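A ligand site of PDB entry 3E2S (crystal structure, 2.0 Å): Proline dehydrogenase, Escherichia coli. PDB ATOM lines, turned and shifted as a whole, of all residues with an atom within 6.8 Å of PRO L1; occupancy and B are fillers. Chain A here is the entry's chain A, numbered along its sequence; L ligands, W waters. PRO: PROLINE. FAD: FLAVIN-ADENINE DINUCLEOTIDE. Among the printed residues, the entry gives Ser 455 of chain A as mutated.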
ATOM      1  N   ASP A 200       1.804  -6.342 -31.531  1.00  0.00           N
ATOM      2  CA  ASP A 200       0.834  -7.380 -31.216  1.00  0.00           C
ATOM      3  C   ASP A 200      -0.006  -7.644 -32.453  1.00  0.00           C
ATOM      4  O   ASP A 200      -0.970  -6.916 -32.731  1.00  0.00           O
ATOM      5  CB  ASP A 200      -0.027  -6.881 -30.057  1.00  0.00           C
ATOM      6  CG  ASP A 200      -1.247  -7.754 -29.782  1.00  0.00           C
ATOM      7  OD1 ASP A 200      -1.338  -8.889 -30.318  1.00  0.00           O
ATOM      8  OD2 ASP A 200      -2.133  -7.299 -29.006  1.00  0.00           O
ATOM      9  N   LEU A 202      -2.730  -8.858 -34.286  1.00  0.00           N
ATOM     10  CA  LEU A 202      -4.080  -9.289 -33.879  1.00  0.00           C
ATOM     11  C   LEU A 202      -4.469 -10.601 -34.554  1.00  0.00           C
ATOM     12  O   LEU A 202      -4.085 -10.859 -35.700  1.00  0.00           O
ATOM     13  CB  LEU A 202      -5.112  -8.218 -34.216  1.00  0.00           C
ATOM     14  CG  LEU A 202      -4.972  -6.885 -33.508  1.00  0.00           C
ATOM     15  CD1 LEU A 202      -5.848  -5.830 -34.181  1.00  0.00           C
ATOM     16  CD2 LEU A 202      -5.328  -7.017 -32.049  1.00  0.00           C
ATOM     17  N   GLU A 204      -6.374 -14.557 -33.068  1.00  0.00           N
ATOM     18  CA  GLU A 204      -6.173 -15.531 -31.996  1.00  0.00           C
ATOM     19  C   GLU A 204      -7.160 -16.676 -32.128  1.00  0.00           C
ATOM     20  O   GLU A 204      -8.043 -16.644 -32.998  1.00  0.00           O
ATOM     21  CB  GLU A 204      -6.354 -14.840 -30.637  1.00  0.00           C
ATOM     22  CG  GLU A 204      -7.742 -14.216 -30.449  1.00  0.00           C
ATOM     23  CD  GLU A 204      -7.828 -13.253 -29.280  1.00  0.00           C
ATOM     24  OE1 GLU A 204      -7.229 -12.149 -29.338  1.00  0.00           O
ATOM     25  OE2 GLU A 204      -8.494 -13.585 -28.285  1.00  0.00           O
ATOM     26  N   SER A 242       4.928  -9.550 -29.563  1.00  0.00           N
ATOM     27  CA  SER A 242       4.212 -10.465 -28.684  1.00  0.00           C
ATOM     28  C   SER A 242       3.380 -11.445 -29.508  1.00  0.00           C
ATOM     29  O   SER A 242       2.931 -11.138 -30.622  1.00  0.00           O
ATOM     30  CB  SER A 242       3.337  -9.720 -27.664  1.00  0.00           C
ATOM     31  OG  SER A 242       2.390  -8.902 -28.316  1.00  0.00           O
ATOM     32  N   LYS A 244       0.470 -14.905 -29.319  1.00  0.00           N
ATOM     33  CA  LYS A 244      -0.512 -15.716 -28.610  1.00  0.00           C
ATOM     34  C   LYS A 244      -0.373 -17.165 -29.052  1.00  0.00           C
ATOM     35  O   LYS A 244      -0.431 -17.468 -30.244  1.00  0.00           O
ATOM     36  CB  LYS A 244      -1.928 -15.218 -28.879  1.00  0.00           C
ATOM     37  CG  LYS A 244      -2.335 -13.992 -28.050  1.00  0.00           C
ATOM     38  CD  LYS A 244      -3.763 -13.547 -28.354  1.00  0.00           C
ATOM     39  CE  LYS A 244      -4.292 -12.616 -27.265  1.00  0.00           C
ATOM     40  NZ  LYS A 244      -3.476 -11.364 -27.170  1.00  0.00           N
ATOM     41  N   ASP A 285       2.037 -14.028 -24.669  1.00  0.00           N
ATOM     42  CA  ASP A 285       0.826 -13.503 -24.007  1.00  0.00           C
ATOM     43  C   ASP A 285       0.199 -14.563 -23.122  1.00  0.00           C
ATOM     44  O   ASP A 285       0.326 -15.754 -23.409  1.00  0.00           O
ATOM     45  CB  ASP A 285      -0.209 -13.042 -25.037  1.00  0.00           C
ATOM     46  CG  ASP A 285       0.131 -11.704 -25.669  1.00  0.00           C
ATOM     47  OD1 ASP A 285       1.133 -11.077 -25.276  1.00  0.00           O
ATOM     48  OD2 ASP A 285      -0.620 -11.263 -26.569  1.00  0.00           O
ATOM     49  N   ALA A 286      -0.467 -14.127 -22.050  1.00  0.00           N
ATOM     50  CA  ALA A 286      -1.256 -15.032 -21.239  1.00  0.00           C
ATOM     51  C   ALA A 286      -2.732 -14.920 -21.663  1.00  0.00           C
ATOM     52  O   ALA A 286      -3.232 -13.819 -21.959  1.00  0.00           O
ATOM     53  CB  ALA A 286      -1.086 -14.721 -19.742  1.00  0.00           C
ATOM     54  N   VAL A 317       3.983 -13.302 -19.995  1.00  0.00           N
ATOM     55  CA  VAL A 317       2.990 -12.556 -19.199  1.00  0.00           C
ATOM     56  C   VAL A 317       2.505 -13.397 -18.034  1.00  0.00           C
ATOM     57  O   VAL A 317       2.307 -14.587 -18.180  1.00  0.00           O
ATOM     58  CB  VAL A 317       1.751 -12.150 -20.050  1.00  0.00           C
ATOM     59  CG1 VAL A 317       0.659 -11.519 -19.172  1.00  0.00           C
ATOM     60  CG2 VAL A 317       2.149 -11.195 -21.147  1.00  0.00           C
ATOM     61  N   ARG A 346       6.179  -9.744 -17.926  1.00  0.00           N
ATOM     62  CA  ARG A 346       5.148  -8.716 -17.927  1.00  0.00           C
ATOM     63  C   ARG A 346       4.115  -9.029 -16.866  1.00  0.00           C
ATOM     64  O   ARG A 346       3.400 -10.016 -16.982  1.00  0.00           O
ATOM     65  CB  ARG A 346       4.428  -8.632 -19.274  1.00  0.00           C
ATOM     66  CG  ARG A 346       5.358  -8.293 -20.413  1.00  0.00           C
ATOM     67  CD  ARG A 346       4.629  -8.154 -21.738  1.00  0.00           C
ATOM     68  NE  ARG A 346       5.583  -7.798 -22.790  1.00  0.00           N
ATOM     69  CZ  ARG A 346       5.260  -7.429 -24.022  1.00  0.00           C
ATOM     70  NH1 ARG A 346       3.976  -7.384 -24.390  1.00  0.00           N
ATOM     71  NH2 ARG A 346       6.232  -7.112 -24.880  1.00  0.00           N
ATOM     72  N   ALA A 351      -6.938  -9.727 -18.641  1.00  0.00           N
ATOM     73  CA  ALA A 351      -7.871  -9.200 -19.638  1.00  0.00           C
ATOM     74  C   ALA A 351      -9.167  -9.984 -19.820  1.00  0.00           C
ATOM     75  O   ALA A 351     -10.032  -9.530 -20.586  1.00  0.00           O
ATOM     76  CB  ALA A 351      -7.191  -9.043 -20.991  1.00  0.00           C
ATOM     77  N   TYR A 352      -9.304 -11.136 -19.164  1.00  0.00           N
ATOM     78  CA  TYR A 352     -10.406 -12.057 -19.464  1.00  0.00           C
ATOM     79  C   TYR A 352     -11.343 -12.268 -18.272  1.00  0.00           C
ATOM     80  O   TYR A 352     -11.990 -13.290 -18.174  1.00  0.00           O
ATOM     81  CB  TYR A 352      -9.856 -13.427 -19.910  1.00  0.00           C
ATOM     82  CG  TYR A 352      -8.868 -13.337 -21.062  1.00  0.00           C
ATOM     83  CD1 TYR A 352      -9.241 -13.708 -22.352  1.00  0.00           C
ATOM     84  CD2 TYR A 352      -7.554 -12.884 -20.852  1.00  0.00           C
ATOM     85  CE1 TYR A 352      -8.340 -13.627 -23.416  1.00  0.00           C
ATOM     86  CE2 TYR A 352      -6.643 -12.806 -21.903  1.00  0.00           C
ATOM     87  CZ  TYR A 352      -7.035 -13.172 -23.170  1.00  0.00           C
ATOM     88  OH  TYR A 352      -6.142 -13.067 -24.202  1.00  0.00           O
ATOM     89  N   LEU A 428      -1.244   0.014 -23.088  1.00  0.00           N
ATOM     90  CA  LEU A 428      -1.906  -0.336 -24.343  1.00  0.00           C
ATOM     91  C   LEU A 428      -2.045   0.928 -25.174  1.00  0.00           C
ATOM     92  O   LEU A 428      -2.385   1.993 -24.653  1.00  0.00           O
ATOM     93  CB  LEU A 428      -3.285  -0.987 -24.105  1.00  0.00           C
ATOM     94  CG  LEU A 428      -3.269  -2.311 -23.349  1.00  0.00           C
ATOM     95  CD1 LEU A 428      -4.702  -2.912 -23.224  1.00  0.00           C
ATOM     96  CD2 LEU A 428      -2.336  -3.302 -24.067  1.00  0.00           C
ATOM     97  N   SER A 455       2.198  -1.460 -26.115  1.00  0.00           N
ATOM     98  CA  SER A 455       1.767  -2.585 -26.908  1.00  0.00           C
ATOM     99  C   SER A 455       0.898  -2.075 -28.059  1.00  0.00           C
ATOM    100  O   SER A 455      -0.109  -1.395 -27.856  1.00  0.00           O
ATOM    101  CB  SER A 455       0.988  -3.610 -26.055  1.00  0.00           C
ATOM    102  OG  SER A 455       0.758  -4.802 -26.793  1.00  0.00           O
ATOM    103  N   PRO A 457      -1.287  -2.911 -31.347  1.00  0.00           N
ATOM    104  CA  PRO A 457      -1.978  -3.924 -32.151  1.00  0.00           C
ATOM    105  C   PRO A 457      -1.802  -3.643 -33.641  1.00  0.00           C
ATOM    106  O   PRO A 457      -1.838  -2.493 -34.098  1.00  0.00           O
ATOM    107  CB  PRO A 457      -3.452  -3.770 -31.735  1.00  0.00           C
ATOM    108  CG  PRO A 457      -3.414  -3.157 -30.352  1.00  0.00           C
ATOM    109  CD  PRO A 457      -2.196  -2.211 -30.417  1.00  0.00           C
ATOM    110  N   ALA A 466     -12.056  -9.870 -31.093  1.00  0.00           N
ATOM    111  CA  ALA A 466     -11.859 -10.354 -29.729  1.00  0.00           C
ATOM    112  C   ALA A 466     -11.085  -9.335 -28.869  1.00  0.00           C
ATOM    113  O   ALA A 466     -11.399  -9.134 -27.683  1.00  0.00           O
ATOM    114  CB  ALA A 466     -11.162 -11.705 -29.729  1.00  0.00           C
ATOM    115  N   TYR A 467     -10.101  -8.681 -29.470  1.00  0.00           N
ATOM    116  CA  TYR A 467      -9.304  -7.669 -28.784  1.00  0.00           C
ATOM    117  C   TYR A 467     -10.178  -6.463 -28.411  1.00  0.00           C
ATOM    118  O   TYR A 467     -10.141  -5.960 -27.284  1.00  0.00           O
ATOM    119  CB  TYR A 467      -8.133  -7.223 -29.675  1.00  0.00           C
ATOM    120  CG  TYR A 467      -7.127  -6.275 -29.012  1.00  0.00           C
ATOM    121  CD1 TYR A 467      -5.978  -6.763 -28.397  1.00  0.00           C
ATOM    122  CD2 TYR A 467      -7.324  -4.907 -29.036  1.00  0.00           C
ATOM    123  CE1 TYR A 467      -5.046  -5.891 -27.798  1.00  0.00           C
ATOM    124  CE2 TYR A 467      -6.402  -4.027 -28.442  1.00  0.00           C
ATOM    125  CZ  TYR A 467      -5.273  -4.530 -27.828  1.00  0.00           C
ATOM    126  OH  TYR A 467      -4.392  -3.648 -27.247  1.00  0.00           O
ATOM    127  N   ARG A 470     -12.445  -7.114 -25.465  1.00  0.00           N
ATOM    128  CA  ARG A 470     -11.686  -7.014 -24.225  1.00  0.00           C
ATOM    129  C   ARG A 470     -11.426  -5.544 -23.816  1.00  0.00           C
ATOM    130  O   ARG A 470     -11.478  -5.203 -22.636  1.00  0.00           O
ATOM    131  CB  ARG A 470     -10.377  -7.828 -24.313  1.00  0.00           C
ATOM    132  CG  ARG A 470     -10.650  -9.330 -24.240  1.00  0.00           C
ATOM    133  CD  ARG A 470      -9.387 -10.161 -23.973  1.00  0.00           C
ATOM    134  NE  ARG A 470      -8.404  -9.997 -25.029  1.00  0.00           N
ATOM    135  CZ  ARG A 470      -8.384 -10.709 -26.149  1.00  0.00           C
ATOM    136  NH1 ARG A 470      -9.303 -11.644 -26.371  1.00  0.00           N
ATOM    137  NH2 ARG A 470      -7.435 -10.487 -27.047  1.00  0.00           N
ATOM    138  N   ARG A 471     -11.154  -4.681 -24.799  1.00  0.00           N
ATOM    139  CA  ARG A 471     -10.969  -3.258 -24.516  1.00  0.00           C
ATOM    140  C   ARG A 471     -12.277  -2.581 -24.081  1.00  0.00           C
ATOM    141  O   ARG A 471     -12.274  -1.719 -23.192  1.00  0.00           O
ATOM    142  CB  ARG A 471     -10.346  -2.523 -25.707  1.00  0.00           C
ATOM    143  CG  ARG A 471      -9.008  -3.078 -26.148  1.00  0.00           C
ATOM    144  CD  ARG A 471      -7.885  -2.760 -25.143  1.00  0.00           C
ATOM    145  NE  ARG A 471      -7.792  -3.691 -24.010  1.00  0.00           N
ATOM    146  CZ  ARG A 471      -7.459  -4.972 -24.124  1.00  0.00           C
ATOM    147  NH1 ARG A 471      -7.250  -5.505 -25.327  1.00  0.00           N
ATOM    148  NH2 ARG A 471      -7.356  -5.746 -23.050  1.00  0.00           N
ATOM    149  N   GLU A 474     -12.839  -3.485 -20.474  1.00  0.00           N
ATOM    150  CA  GLU A 474     -11.849  -2.856 -19.602  1.00  0.00           C
ATOM    151  C   GLU A 474     -12.187  -1.386 -19.407  1.00  0.00           C
ATOM    152  O   GLU A 474     -12.210  -0.888 -18.286  1.00  0.00           O
ATOM    153  CB  GLU A 474     -10.443  -2.992 -20.206  1.00  0.00           C
ATOM    154  CG  GLU A 474      -9.303  -2.429 -19.340  1.00  0.00           C
ATOM    155  CD  GLU A 474      -7.929  -2.615 -19.993  1.00  0.00           C
ATOM    156  OE1 GLU A 474      -7.845  -3.311 -21.027  1.00  0.00           O
ATOM    157  OE2 GLU A 474      -6.933  -2.055 -19.472  1.00  0.00           O
HETATM  158  N   PRO L   1      -2.887  -9.128 -24.385  1.00  0.00           N
HETATM  159  CA  PRO L   1      -3.980  -8.302 -24.138  1.00  0.00           C
HETATM  160  C   PRO L   1      -5.144  -8.656 -24.912  1.00  0.00           C
HETATM  161  O   PRO L   1      -5.057  -9.377 -25.864  1.00  0.00           O
HETATM  162  CB  PRO L   1      -3.673  -6.908 -24.319  1.00  0.00           C
HETATM  163  CG  PRO L   1      -2.530  -6.897 -25.316  1.00  0.00           C
HETATM  164  CD  PRO L   1      -2.297  -8.354 -25.655  1.00  0.00           C
HETATM  165  OXT PRO L   1      -6.219  -8.245 -24.598  1.00  0.00           O
HETATM  166  PA  FAD L   2      -7.178  -1.217 -13.255  1.00  0.00           P
HETATM  167  O1A FAD L   2      -8.559  -0.347 -13.485  1.00  0.00           O
HETATM  168  O2A FAD L   2      -6.449  -0.773 -12.076  1.00  0.00           O
HETATM  169  O5B FAD L   2      -7.607  -2.770 -13.047  1.00  0.00           O
HETATM  170  C5B FAD L   2      -8.411  -3.305 -14.064  1.00  0.00           C
HETATM  171  C4B FAD L   2      -8.878  -4.730 -13.852  1.00  0.00           C
HETATM  172  O4B FAD L   2      -8.798  -5.431 -12.619  1.00  0.00           O
HETATM  173  C3B FAD L   2      -9.066  -5.718 -14.850  1.00  0.00           C
HETATM  174  O3B FAD L   2      -8.784  -5.500 -16.195  1.00  0.00           O
HETATM  175  C2B FAD L   2      -8.953  -6.960 -14.187  1.00  0.00           C
HETATM  176  O2B FAD L   2      -7.892  -7.816 -14.472  1.00  0.00           O
HETATM  177  C1B FAD L   2      -9.370  -6.677 -12.844  1.00  0.00           C
HETATM  178  N9A FAD L   2     -10.703  -6.845 -12.325  1.00  0.00           N
HETATM  179  C8A FAD L   2     -11.750  -6.090 -12.695  1.00  0.00           C
HETATM  180  N7A FAD L   2     -12.824  -6.433 -11.901  1.00  0.00           N
HETATM  181  C5A FAD L   2     -12.400  -7.400 -11.021  1.00  0.00           C
HETATM  182  C6A FAD L   2     -13.060  -8.066 -10.034  1.00  0.00           C
HETATM  183  N6A FAD L   2     -14.478  -7.801  -9.770  1.00  0.00           N
HETATM  184  N1A FAD L   2     -12.421  -8.974  -9.311  1.00  0.00           N
HETATM  185  C2A FAD L   2     -11.112  -9.248  -9.552  1.00  0.00           C
HETATM  186  N3A FAD L   2     -10.452  -8.590 -10.533  1.00  0.00           N
HETATM  187  C4A FAD L   2     -11.101  -7.660 -11.259  1.00  0.00           C
HETATM  188  N1  FAD L   2      -3.954  -9.161 -20.062  1.00  0.00           N
HETATM  189  C2  FAD L   2      -4.023 -10.490 -20.195  1.00  0.00           C
HETATM  190  O2  FAD L   2      -4.953 -11.225 -19.471  1.00  0.00           O
HETATM  191  N3  FAD L   2      -3.056 -11.200 -20.893  1.00  0.00           N
HETATM  192  C4  FAD L   2      -2.010 -10.520 -21.478  1.00  0.00           C
HETATM  193  O4  FAD L   2      -1.075 -11.245 -22.213  1.00  0.00           O
HETATM  194  C4X FAD L   2      -1.911  -9.155 -21.349  1.00  0.00           C
HETATM  195  N5  FAD L   2      -0.876  -8.491 -21.922  1.00  0.00           N
HETATM  196  C5X FAD L   2      -0.778  -7.174 -21.806  1.00  0.00           C
HETATM  197  C6  FAD L   2       0.280  -6.421 -22.347  1.00  0.00           C
HETATM  198  C7  FAD L   2       0.321  -5.025 -22.175  1.00  0.00           C
HETATM  199  C7M FAD L   2       1.477  -4.218 -22.763  1.00  0.00           C
HETATM  200  C8  FAD L   2      -0.677  -4.381 -21.464  1.00  0.00           C
HETATM  201  C8M FAD L   2      -0.631  -2.878 -21.186  1.00  0.00           C
HETATM  202  C9  FAD L   2      -1.704  -5.120 -20.922  1.00  0.00           C
HETATM  203  C9A FAD L   2      -1.725  -6.501 -21.106  1.00  0.00           C
HETATM  204  N10 FAD L   2      -2.732  -7.147 -20.561  1.00  0.00           N
HETATM  205  C10 FAD L   2      -2.869  -8.474 -20.655  1.00  0.00           C
HETATM  206  C1' FAD L   2      -3.707  -6.196 -20.138  1.00  0.00           C
HETATM  207  C2' FAD L   2      -4.419  -6.287 -18.847  1.00  0.00           C
HETATM  208  O2' FAD L   2      -4.395  -7.282 -18.206  1.00  0.00           O
HETATM  209  C3' FAD L   2      -5.371  -5.123 -18.640  1.00  0.00           C
HETATM  210  O3' FAD L   2      -5.017  -3.971 -19.382  1.00  0.00           O
HETATM  211  C4' FAD L   2      -5.452  -4.855 -17.162  1.00  0.00           C
HETATM  212  O4' FAD L   2      -5.925  -5.928 -16.412  1.00  0.00           O
HETATM  213  C5' FAD L   2      -5.771  -3.432 -16.717  1.00  0.00           C
HETATM  214  O5' FAD L   2      -5.103  -3.151 -15.535  1.00  0.00           O
HETATM  215  P   FAD L   2      -4.939  -1.612 -15.050  1.00  0.00           P
HETATM  216  O1P FAD L   2      -3.968  -1.616 -13.738  1.00  0.00           O
HETATM  217  O2P FAD L   2      -4.491  -0.757 -16.148  1.00  0.00           O
HETATM  218  O3P FAD L   2      -6.451  -1.034 -14.706  1.00  0.00           O
HETATM  219  O   HOH W   1      -1.671  -4.701 -27.797  1.00  0.00           O
HETATM  220  O   HOH W   2      -3.573 -11.802 -24.083  1.00  0.00           O
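Residues that only touch PRO L1: Asp 200 (3.5 Å), Ala 351 (3.8 Å), Leu 428 (3.8 Å) and Tyr 467 (3.7 Å). Eight residues have an atom within 4 Å of PRO L1: Asp 200, Lys 244, Asp 285, Ala 351, Leu 428, Tyr 467, Arg 470 and Arg 471. The nearest printed residue that does not touch PRO L1 is Ser 455 (4.2 Å).
N of PRO L1 sits close to N5 of FAD L2.
Water W2 lies within hydrogen-bond range of N of PRO L1 (2.8 Å), OH of Tyr 352 (2.9 Å), O of Ala 286 (2.9 Å), NZ of Lys 244 (3.1 Å) and O4 of FAD L2 (3.2 Å). Water W1 lies within hydrogen-bond range of OG of Ser 455 (2.6 Å), OD2 of Asp 200 (2.9 Å) and OH of Tyr 467 (3.0 Å).
The guanidinium group of Arg 470 lies within salt-bridge range of an oxygen (OXT) of PRO L1, at 2.8 Å. The side-chain amino group (NZ) of Lys 244 lies within salt-bridge range of an oxygen (O) of PRO L1 (2.9 Å). The guanidinium group (NH1) of Arg 471 is in salt-bridge range of an oxygen (OXT) of PRO L1 (3.0 Å). OD2 of Asp 285 is in salt-bridge range of N of PRO L1 (3.8 Å). The backbone NH (N) of Ala 351 sits at hydrogen-bond distance from an oxygen (O2) of FAD L2 (2.6 Å). An oxygen (O4) of FAD L2 is in hydrogen-bond range of the backbone NH (N) of Ala 286. A nitrogen (N3) of FAD L2 is in hydrogen-bond range of the backbone carbonyl oxygen (O) of Ala 286. OE2 of Glu 474 is in hydrogen-bond range of O3' of FAD L2 (2.7 Å).
OE1 of Glu 204 lies within salt-bridge range of NH2 of Arg 470 (2.8 Å). NZ of Lys 244 lies within salt-bridge range of OD2 of Asp 285, 2.9 Å away. NE of Arg 471 is in salt-bridge range of OE1 of Glu 474 (3.0 Å).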
